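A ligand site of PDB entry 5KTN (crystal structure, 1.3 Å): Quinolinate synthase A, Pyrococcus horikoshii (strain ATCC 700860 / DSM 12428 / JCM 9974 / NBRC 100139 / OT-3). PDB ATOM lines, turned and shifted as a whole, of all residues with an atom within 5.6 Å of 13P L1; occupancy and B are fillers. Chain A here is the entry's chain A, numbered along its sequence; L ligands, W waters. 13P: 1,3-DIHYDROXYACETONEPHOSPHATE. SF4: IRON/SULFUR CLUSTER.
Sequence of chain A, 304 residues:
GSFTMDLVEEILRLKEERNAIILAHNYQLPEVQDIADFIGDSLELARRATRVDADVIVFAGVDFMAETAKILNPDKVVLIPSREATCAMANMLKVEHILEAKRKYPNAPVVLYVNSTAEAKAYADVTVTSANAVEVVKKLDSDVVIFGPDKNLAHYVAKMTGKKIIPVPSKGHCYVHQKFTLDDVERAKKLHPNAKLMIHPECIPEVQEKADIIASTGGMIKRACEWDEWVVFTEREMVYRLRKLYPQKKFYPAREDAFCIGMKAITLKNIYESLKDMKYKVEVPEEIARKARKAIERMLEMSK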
ATOM      1  N   HIS A  25       5.335 -25.196 -35.054  1.00  0.00           N
ATOM      2  CA  HIS A  25       5.874 -24.987 -33.716  1.00  0.00           C
ATOM      3  C   HIS A  25       7.270 -25.612 -33.598  1.00  0.00           C
ATOM      4  O   HIS A  25       7.634 -26.550 -34.321  1.00  0.00           O
ATOM      5  CB  HIS A  25       4.953 -25.600 -32.660  1.00  0.00           C
ATOM      6  CG  HIS A  25       5.375 -25.262 -31.266  1.00  0.00           C
ATOM      7  ND1 HIS A  25       6.117 -26.129 -30.497  1.00  0.00           N
ATOM      8  CD2 HIS A  25       5.207 -24.141 -30.528  1.00  0.00           C
ATOM      9  CE1 HIS A  25       6.375 -25.560 -29.328  1.00  0.00           C
ATOM     10  NE2 HIS A  25       5.830 -24.351 -29.323  1.00  0.00           N
ATOM     11  N   ASN A  26       8.030 -25.085 -32.621  1.00  0.00           N
ATOM     12  CA  ASN A  26       9.382 -25.555 -32.328  1.00  0.00           C
ATOM     13  C   ASN A  26       9.486 -27.040 -31.980  1.00  0.00           C
ATOM     14  O   ASN A  26      10.588 -27.600 -32.050  1.00  0.00           O
ATOM     15  CB  ASN A  26       9.957 -24.735 -31.163  1.00  0.00           C
ATOM     16  CG  ASN A  26      10.278 -23.316 -31.566  1.00  0.00           C
ATOM     17  OD1 ASN A  26      10.742 -23.067 -32.681  1.00  0.00           O
ATOM     18  ND2 ASN A  26      10.040 -22.366 -30.650  1.00  0.00           N
ATOM     19  N   TYR A  27       8.385 -27.709 -31.600  1.00  0.00           N
ATOM     20  CA  TYR A  27       8.437 -29.117 -31.229  1.00  0.00           C
ATOM     21  C   TYR A  27       8.133 -30.042 -32.407  1.00  0.00           C
ATOM     22  O   TYR A  27       8.044 -31.264 -32.217  1.00  0.00           O
ATOM     23  CB  TYR A  27       7.440 -29.439 -30.108  1.00  0.00           C
ATOM     24  CG  TYR A  27       7.638 -28.715 -28.788  1.00  0.00           C
ATOM     25  CD1 TYR A  27       8.838 -28.089 -28.465  1.00  0.00           C
ATOM     26  CD2 TYR A  27       6.605 -28.671 -27.855  1.00  0.00           C
ATOM     27  CE1 TYR A  27       9.001 -27.432 -27.244  1.00  0.00           C
ATOM     28  CE2 TYR A  27       6.747 -28.029 -26.644  1.00  0.00           C
ATOM     29  CZ  TYR A  27       7.936 -27.404 -26.338  1.00  0.00           C
ATOM     30  OH  TYR A  27       8.031 -26.755 -25.118  1.00  0.00           O
ATOM     31  N   GLY A  40       8.035 -21.103 -34.806  1.00  0.00           N
ATOM     32  CA  GLY A  40       8.123 -20.265 -33.616  1.00  0.00           C
ATOM     33  C   GLY A  40       7.448 -20.882 -32.413  1.00  0.00           C
ATOM     34  O   GLY A  40       6.953 -22.014 -32.455  1.00  0.00           O
ATOM     35  N   ASP A  41       7.426 -20.106 -31.331  1.00  0.00           N
ATOM     36  CA  ASP A  41       6.750 -20.503 -30.100  1.00  0.00           C
ATOM     37  C   ASP A  41       5.280 -20.078 -30.183  1.00  0.00           C
ATOM     38  O   ASP A  41       4.833 -19.527 -31.189  1.00  0.00           O
ATOM     39  CB  ASP A  41       7.504 -19.996 -28.866  1.00  0.00           C
ATOM     40  CG  ASP A  41       7.310 -18.517 -28.576  1.00  0.00           C
ATOM     41  OD1 ASP A  41       6.745 -17.783 -29.417  1.00  0.00           O
ATOM     42  OD2 ASP A  41       7.746 -18.090 -27.467  1.00  0.00           O
ATOM     43  N   SER A  42       4.527 -20.332 -29.116  1.00  0.00           N
ATOM     44  CA  SER A  42       3.089 -20.071 -29.161  1.00  0.00           C
ATOM     45  C   SER A  42       2.796 -18.594 -29.406  1.00  0.00           C
ATOM     46  O   SER A  42       1.933 -18.248 -30.220  1.00  0.00           O
ATOM     47  CB  SER A  42       2.420 -20.571 -27.900  1.00  0.00           C
ATOM     48  OG  SER A  42       1.019 -20.403 -27.972  1.00  0.00           O
ATOM     49  N   LEU A  43       3.505 -17.693 -28.715  1.00  0.00           N
ATOM     50  CA  LEU A  43       3.264 -16.273 -28.899  1.00  0.00           C
ATOM     51  C   LEU A  43       3.663 -15.811 -30.293  1.00  0.00           C
ATOM     52  O   LEU A  43       2.955 -15.018 -30.917  1.00  0.00           O
ATOM     53  CB  LEU A  43       4.013 -15.461 -27.839  1.00  0.00           C
ATOM     54  CG  LEU A  43       3.866 -13.937 -27.929  1.00  0.00           C
ATOM     55  CD1 LEU A  43       2.403 -13.500 -27.907  1.00  0.00           C
ATOM     56  CD2 LEU A  43       4.623 -13.298 -26.792  1.00  0.00           C
ATOM     57  N   PHE A  64      -4.965 -26.293 -30.241  1.00  0.00           N
ATOM     58  CA  PHE A  64      -5.202 -24.952 -29.706  1.00  0.00           C
ATOM     59  C   PHE A  64      -4.441 -23.899 -30.505  1.00  0.00           C
ATOM     60  O   PHE A  64      -4.892 -22.752 -30.611  1.00  0.00           O
ATOM     61  CB  PHE A  64      -4.931 -24.869 -28.190  1.00  0.00           C
ATOM     62  CG  PHE A  64      -3.452 -24.829 -27.808  1.00  0.00           C
ATOM     63  CD1 PHE A  64      -2.713 -23.650 -27.904  1.00  0.00           C
ATOM     64  CD2 PHE A  64      -2.834 -25.964 -27.320  1.00  0.00           C
ATOM     65  CE1 PHE A  64      -1.389 -23.622 -27.539  1.00  0.00           C
ATOM     66  CE2 PHE A  64      -1.497 -25.942 -26.950  1.00  0.00           C
ATOM     67  CZ  PHE A  64      -0.768 -24.777 -27.065  1.00  0.00           C
ATOM     68  N   MET A  65      -3.300 -24.273 -31.080  1.00  0.00           N
ATOM     69  CA  MET A  65      -2.534 -23.340 -31.896  1.00  0.00           C
ATOM     70  C   MET A  65      -3.228 -23.090 -33.234  1.00  0.00           C
ATOM     71  O   MET A  65      -3.332 -21.933 -33.669  1.00  0.00           O
ATOM     72  CB  MET A  65      -1.127 -23.880 -32.110  1.00  0.00           C
ATOM     73  CG  MET A  65      -0.359 -24.066 -30.809  1.00  0.00           C
ATOM     74  SD  MET A  65       1.280 -24.744 -31.119  1.00  0.00           S
ATOM     75  CE  MET A  65       1.907 -24.795 -29.433  1.00  0.00           C
ATOM     76  N   TYR A 113      -4.002 -19.263 -20.326  1.00  0.00           N
ATOM     77  CA  TYR A 113      -2.927 -19.732 -21.183  1.00  0.00           C
ATOM     78  C   TYR A 113      -3.498 -19.999 -22.561  1.00  0.00           C
ATOM     79  O   TYR A 113      -4.629 -20.483 -22.699  1.00  0.00           O
ATOM     80  CB  TYR A 113      -2.399 -21.047 -20.600  1.00  0.00           C
ATOM     81  CG  TYR A 113      -0.948 -21.385 -20.829  1.00  0.00           C
ATOM     82  CD1 TYR A 113      -0.050 -20.493 -21.421  1.00  0.00           C
ATOM     83  CD2 TYR A 113      -0.460 -22.614 -20.436  1.00  0.00           C
ATOM     84  CE1 TYR A 113       1.273 -20.838 -21.612  1.00  0.00           C
ATOM     85  CE2 TYR A 113       0.853 -22.968 -20.632  1.00  0.00           C
ATOM     86  CZ  TYR A 113       1.710 -22.083 -21.208  1.00  0.00           C
ATOM     87  OH  TYR A 113       3.021 -22.475 -21.380  1.00  0.00           O
ATOM     88  N   ASN A 115      -2.772 -22.397 -24.313  1.00  0.00           N
ATOM     89  CA  ASN A 115      -3.123 -23.817 -24.214  1.00  0.00           C
ATOM     90  C   ASN A 115      -4.500 -23.921 -23.558  1.00  0.00           C
ATOM     91  O   ASN A 115      -4.620 -24.196 -22.361  1.00  0.00           O
ATOM     92  CB  ASN A 115      -2.104 -24.589 -23.376  1.00  0.00           C
ATOM     93  CG  ASN A 115      -0.667 -24.369 -23.830  1.00  0.00           C
ATOM     94  OD1 ASN A 115      -0.212 -23.235 -24.002  1.00  0.00           O
ATOM     95  ND2 ASN A 115       0.056 -25.471 -24.014  1.00  0.00           N
ATOM     96  N   THR A 129       0.966 -16.505 -23.019  1.00  0.00           N
ATOM     97  CA  THR A 129       1.816 -17.674 -23.216  1.00  0.00           C
ATOM     98  C   THR A 129       2.920 -17.609 -22.173  1.00  0.00           C
ATOM     99  O   THR A 129       3.012 -16.659 -21.382  1.00  0.00           O
ATOM    100  CB  THR A 129       2.443 -17.746 -24.623  1.00  0.00           C
ATOM    101  OG1 THR A 129       3.571 -16.876 -24.695  1.00  0.00           O
ATOM    102  CG2 THR A 129       1.419 -17.362 -25.679  1.00  0.00           C
ATOM    103  N   SER A 130       3.795 -18.620 -22.205  1.00  0.00           N
ATOM    104  CA  SER A 130       4.919 -18.626 -21.284  1.00  0.00           C
ATOM    105  C   SER A 130       5.867 -17.454 -21.521  1.00  0.00           C
ATOM    106  O   SER A 130       6.669 -17.134 -20.634  1.00  0.00           O
ATOM    107  CB  SER A 130       5.698 -19.932 -21.435  1.00  0.00           C
ATOM    108  OG  SER A 130       5.999 -20.146 -22.794  1.00  0.00           O
ATOM    109  N   ALA A 131       5.804 -16.813 -22.687  1.00  0.00           N
ATOM    110  CA  ALA A 131       6.692 -15.698 -23.004  1.00  0.00           C
ATOM    111  C   ALA A 131       6.241 -14.387 -22.399  1.00  0.00           C
ATOM    112  O   ALA A 131       7.071 -13.494 -22.175  1.00  0.00           O
ATOM    113  CB  ALA A 131       6.786 -15.545 -24.522  1.00  0.00           C
ATOM    114  N   CYS A 174       1.459 -30.148 -17.784  1.00  0.00           N
ATOM    115  CA  CYS A 174       1.905 -30.788 -19.004  1.00  0.00           C
ATOM    116  C   CYS A 174       2.707 -32.040 -18.664  1.00  0.00           C
ATOM    117  O   CYS A 174       3.756 -31.944 -18.006  1.00  0.00           O
ATOM    118  CB  CYS A 174       2.794 -29.819 -19.793  1.00  0.00           C
ATOM    119  SG  CYS A 174       3.727 -30.632 -21.125  1.00  0.00           S
ATOM    120  N   HIS A 177       6.605 -31.917 -19.672  1.00  0.00           N
ATOM    121  CA  HIS A 177       7.504 -31.181 -18.797  1.00  0.00           C
ATOM    122  C   HIS A 177       7.568 -31.753 -17.390  1.00  0.00           C
ATOM    123  O   HIS A 177       8.575 -31.563 -16.715  1.00  0.00           O
ATOM    124  CB  HIS A 177       7.167 -29.689 -18.820  1.00  0.00           C
ATOM    125  CG  HIS A 177       7.521 -29.042 -20.121  1.00  0.00           C
ATOM    126  ND1 HIS A 177       6.643 -28.967 -21.181  1.00  0.00           N
ATOM    127  CD2 HIS A 177       8.686 -28.494 -20.558  1.00  0.00           C
ATOM    128  CE1 HIS A 177       7.240 -28.380 -22.200  1.00  0.00           C
ATOM    129  NE2 HIS A 177       8.483 -28.089 -21.850  1.00  0.00           N
ATOM    130  N   HIS A 200      11.910 -24.610 -19.255  1.00  0.00           N
ATOM    131  CA  HIS A 200      10.587 -24.099 -19.556  1.00  0.00           C
ATOM    132  C   HIS A 200       9.783 -23.940 -18.257  1.00  0.00           C
ATOM    133  O   HIS A 200       9.882 -24.778 -17.358  1.00  0.00           O
ATOM    134  CB  HIS A 200       9.857 -25.079 -20.485  1.00  0.00           C
ATOM    135  CG  HIS A 200       8.732 -24.453 -21.230  1.00  0.00           C
ATOM    136  ND1 HIS A 200       7.495 -24.226 -20.676  1.00  0.00           N
ATOM    137  CD2 HIS A 200       8.683 -23.944 -22.491  1.00  0.00           C
ATOM    138  CE1 HIS A 200       6.708 -23.647 -21.562  1.00  0.00           C
ATOM    139  NE2 HIS A 200       7.412 -23.453 -22.670  1.00  0.00           N
ATOM    140  N   GLU A 202       6.809 -24.630 -17.706  1.00  0.00           N
ATOM    141  CA  GLU A 202       5.920 -25.765 -17.472  1.00  0.00           C
ATOM    142  C   GLU A 202       6.585 -26.856 -16.642  1.00  0.00           C
ATOM    143  O   GLU A 202       5.896 -27.790 -16.215  1.00  0.00           O
ATOM    144  CB  GLU A 202       5.372 -26.307 -18.796  1.00  0.00           C
ATOM    145  CG  GLU A 202       4.392 -25.337 -19.477  1.00  0.00           C
ATOM    146  CD  GLU A 202       4.044 -25.742 -20.898  1.00  0.00           C
ATOM    147  OE1 GLU A 202       4.399 -26.874 -21.280  1.00  0.00           O
ATOM    148  OE2 GLU A 202       3.425 -24.934 -21.630  1.00  0.00           O
ATOM    149  N   ALA A 215      12.342 -19.719 -19.514  1.00  0.00           N
ATOM    150  CA  ALA A 215      11.867 -19.044 -20.717  1.00  0.00           C
ATOM    151  C   ALA A 215      10.922 -19.939 -21.503  1.00  0.00           C
ATOM    152  O   ALA A 215      11.024 -21.165 -21.440  1.00  0.00           O
ATOM    153  CB  ALA A 215      13.050 -18.648 -21.613  1.00  0.00           C
ATOM    154  N   SER A 216      10.029 -19.303 -22.246  1.00  0.00           N
ATOM    155  CA  SER A 216       9.327 -19.977 -23.323  1.00  0.00           C
ATOM    156  C   SER A 216      10.344 -20.495 -24.335  1.00  0.00           C
ATOM    157  O   SER A 216      11.518 -20.122 -24.323  1.00  0.00           O
ATOM    158  CB  SER A 216       8.393 -18.998 -24.036  1.00  0.00           C
ATOM    159  OG  SER A 216       9.131 -18.078 -24.832  1.00  0.00           O
ATOM    160  N   THR A 217       9.884 -21.361 -25.252  1.00  0.00           N
ATOM    161  CA  THR A 217      10.816 -21.802 -26.290  1.00  0.00           C
ATOM    162  C   THR A 217      11.294 -20.625 -27.139  1.00  0.00           C
ATOM    163  O   THR A 217      12.459 -20.602 -27.569  1.00  0.00           O
ATOM    164  CB  THR A 217      10.218 -22.921 -27.154  1.00  0.00           C
ATOM    165  OG1 THR A 217       9.106 -22.429 -27.908  1.00  0.00           O
ATOM    166  CG2 THR A 217       9.778 -24.122 -26.307  1.00  0.00           C
ATOM    167  N   GLY A 218      10.450 -19.614 -27.345  1.00  0.00           N
ATOM    168  CA  GLY A 218      10.887 -18.420 -28.057  1.00  0.00           C
ATOM    169  C   GLY A 218      11.964 -17.685 -27.290  1.00  0.00           C
ATOM    170  O   GLY A 218      12.940 -17.205 -27.877  1.00  0.00           O
ATOM    171  N   THR A 234      13.146 -28.902 -22.140  1.00  0.00           N
ATOM    172  CA  THR A 234      11.837 -28.842 -22.791  1.00  0.00           C
ATOM    173  C   THR A 234      11.741 -30.027 -23.751  1.00  0.00           C
ATOM    174  O   THR A 234      12.625 -30.885 -23.787  1.00  0.00           O
ATOM    175  CB  THR A 234      11.552 -27.462 -23.404  1.00  0.00           C
ATOM    176  OG1 THR A 234      10.164 -27.364 -23.761  1.00  0.00           O
ATOM    177  CG2 THR A 234      12.402 -27.193 -24.632  1.00  0.00           C
ATOM    178  N   MET A 263       2.104 -33.166 -30.704  1.00  0.00           N
ATOM    179  CA  MET A 263       2.957 -32.540 -31.702  1.00  0.00           C
ATOM    180  C   MET A 263       3.371 -33.543 -32.772  1.00  0.00           C
ATOM    181  O   MET A 263       3.368 -33.220 -33.970  1.00  0.00           O
ATOM    182  CB  MET A 263       4.190 -31.946 -31.029  1.00  0.00           C
ATOM    183  CG  MET A 263       3.886 -30.682 -30.258  1.00  0.00           C
ATOM    184  SD  MET A 263       3.523 -29.290 -31.371  1.00  0.00           S
ATOM    185  CE  MET A 263       3.211 -27.986 -30.161  1.00  0.00           C
HETATM  186  P   13P L   1       6.023 -22.206 -25.986  1.00  0.00           P
HETATM  187  O1P 13P L   1       6.528 -22.698 -27.305  1.00  0.00           O
HETATM  188  O2P 13P L   1       5.074 -20.950 -26.131  1.00  0.00           O
HETATM  189  O3P 13P L   1       7.210 -21.918 -24.972  1.00  0.00           O
HETATM  190  O1  13P L   1       5.190 -23.363 -25.249  1.00  0.00           O
HETATM  191  C1  13P L   1       4.283 -24.037 -26.105  1.00  0.00           C
HETATM  192  C2  13P L   1       4.014 -25.380 -25.459  1.00  0.00           C
HETATM  193  O2  13P L   1       3.171 -26.215 -26.059  1.00  0.00           O
HETATM  194  C3  13P L   1       4.882 -25.866 -24.396  1.00  0.00           C
HETATM  195  O3  13P L   1       4.560 -27.081 -23.881  1.00  0.00           O
HETATM  196 FE1  SF4 L   2       0.541 -29.430 -24.563  1.00  0.00          FE
HETATM  197 FE2  SF4 L   2       2.435 -30.917 -25.811  1.00  0.00          FE
HETATM  198 FE3  SF4 L   2       2.681 -30.272 -23.164  1.00  0.00          FE
HETATM  199 FE4  SF4 L   2       2.993 -28.237 -24.903  1.00  0.00          FE
HETATM  200  S1  SF4 L   2       4.297 -30.197 -24.763  1.00  0.00           S
HETATM  201  S2  SF4 L   2       1.690 -28.241 -23.020  1.00  0.00           S
HETATM  202  S3  SF4 L   2       1.456 -29.016 -26.554  1.00  0.00           S
HETATM  203  S4  SF4 L   2       1.060 -31.619 -24.068  1.00  0.00           S
HETATM  204  O   HOH W   1       2.371 -23.785 -23.607  1.00  0.00           O
HETATM  205  O   HOH W   2       5.194 -18.374 -26.327  1.00  0.00           O
HETATM  206  O   HOH W   3       3.363 -20.970 -23.999  1.00  0.00           O
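OE1 of Glu 202 lies close to O3 of 13P L1, 2.6 Å away. N of Thr 217 is in hydrogen-bond range of O3P of 13P L1 (2.7 Å). OG1 of Thr 217 is in hydrogen-bond range of O1P of 13P L1, 2.7 Å away. NE2 of His 25 lies within hydrogen-bond range of O1P of 13P L1. A ring nitrogen (NE2) of His 200 sits at hydrogen-bond distance from an oxygen (O3P) of 13P L1, 2.8 Å away. The side-chain hydroxyl (OG) of Ser 130 sits at hydrogen-bond distance from an oxygen (O3P) of 13P L1 (3.1 Å). An oxygen (O2P) of 13P L1 is in hydrogen-bond range of the backbone NH (N) of Ser 42 (3.1 Å). ND2 of Asn 115 sits close to S2 of SF4 L2, 3.4 Å away. FE3 of SF4 L2 is bound by SG of Cys 174 (2.3 Å).
Water W2 lies within hydrogen-bond range of O2P of 13P L1 (2.6 Å), OG1 of Thr 129 (2.7 Å), OD2 of Asp 41 (2.8 Å), N of Leu 43 (3.0 Å) and N of Ser 42 (3.5 Å). Water W3 lies within hydrogen-bond range of an oxygen (O2P) of 13P L1 (2.7 Å), the backbone NH (N) of Ser 130 (3.0 Å) and the side-chain hydroxyl (OH) of Tyr 113 (3.0 Å).
O3 of 13P L1 is bound to FE4 of SF4 L2.
Residues that only touch 13P L1: Asp 41, Ser 216, Tyr 27, His 177, Asn 115 and Met 65. Hydrophobic or aromatic side chains that line 13P L1: His 25, Tyr 27, Met 65, His 177 and His 200.
The side-chain carboxylate of Glu 202 sits at hydrogen-bond distance from a ring nitrogen (ND1) of His 177. The backbone NH (N) of Tyr 27 sits at hydrogen-bond distance from a ring nitrogen (ND1) of His 25, 3.0 Å away. N of Leu 43 lies close to OD1 of Asp 41, at 3.3 Å. The side-chain carboxylate of Asp 41 sits at hydrogen-bond distance from the backbone NH of Gly 218, at 3.1 Å. OG of Ser 216 lies close to N of Gly 218 (3.2 Å). The side-chain hydroxyl (OH) of Tyr 27 lies within hydrogen-bond range of the side-chain hydroxyl (OG1) of Thr 234 (2.6 Å). A ring nitrogen (ND1) of His 177 sits close to the side-chain sulfur of Cys 174 (3.4 Å). NE2 of His 177 lies within hydrogen-bond range of OG1 of Thr 234.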
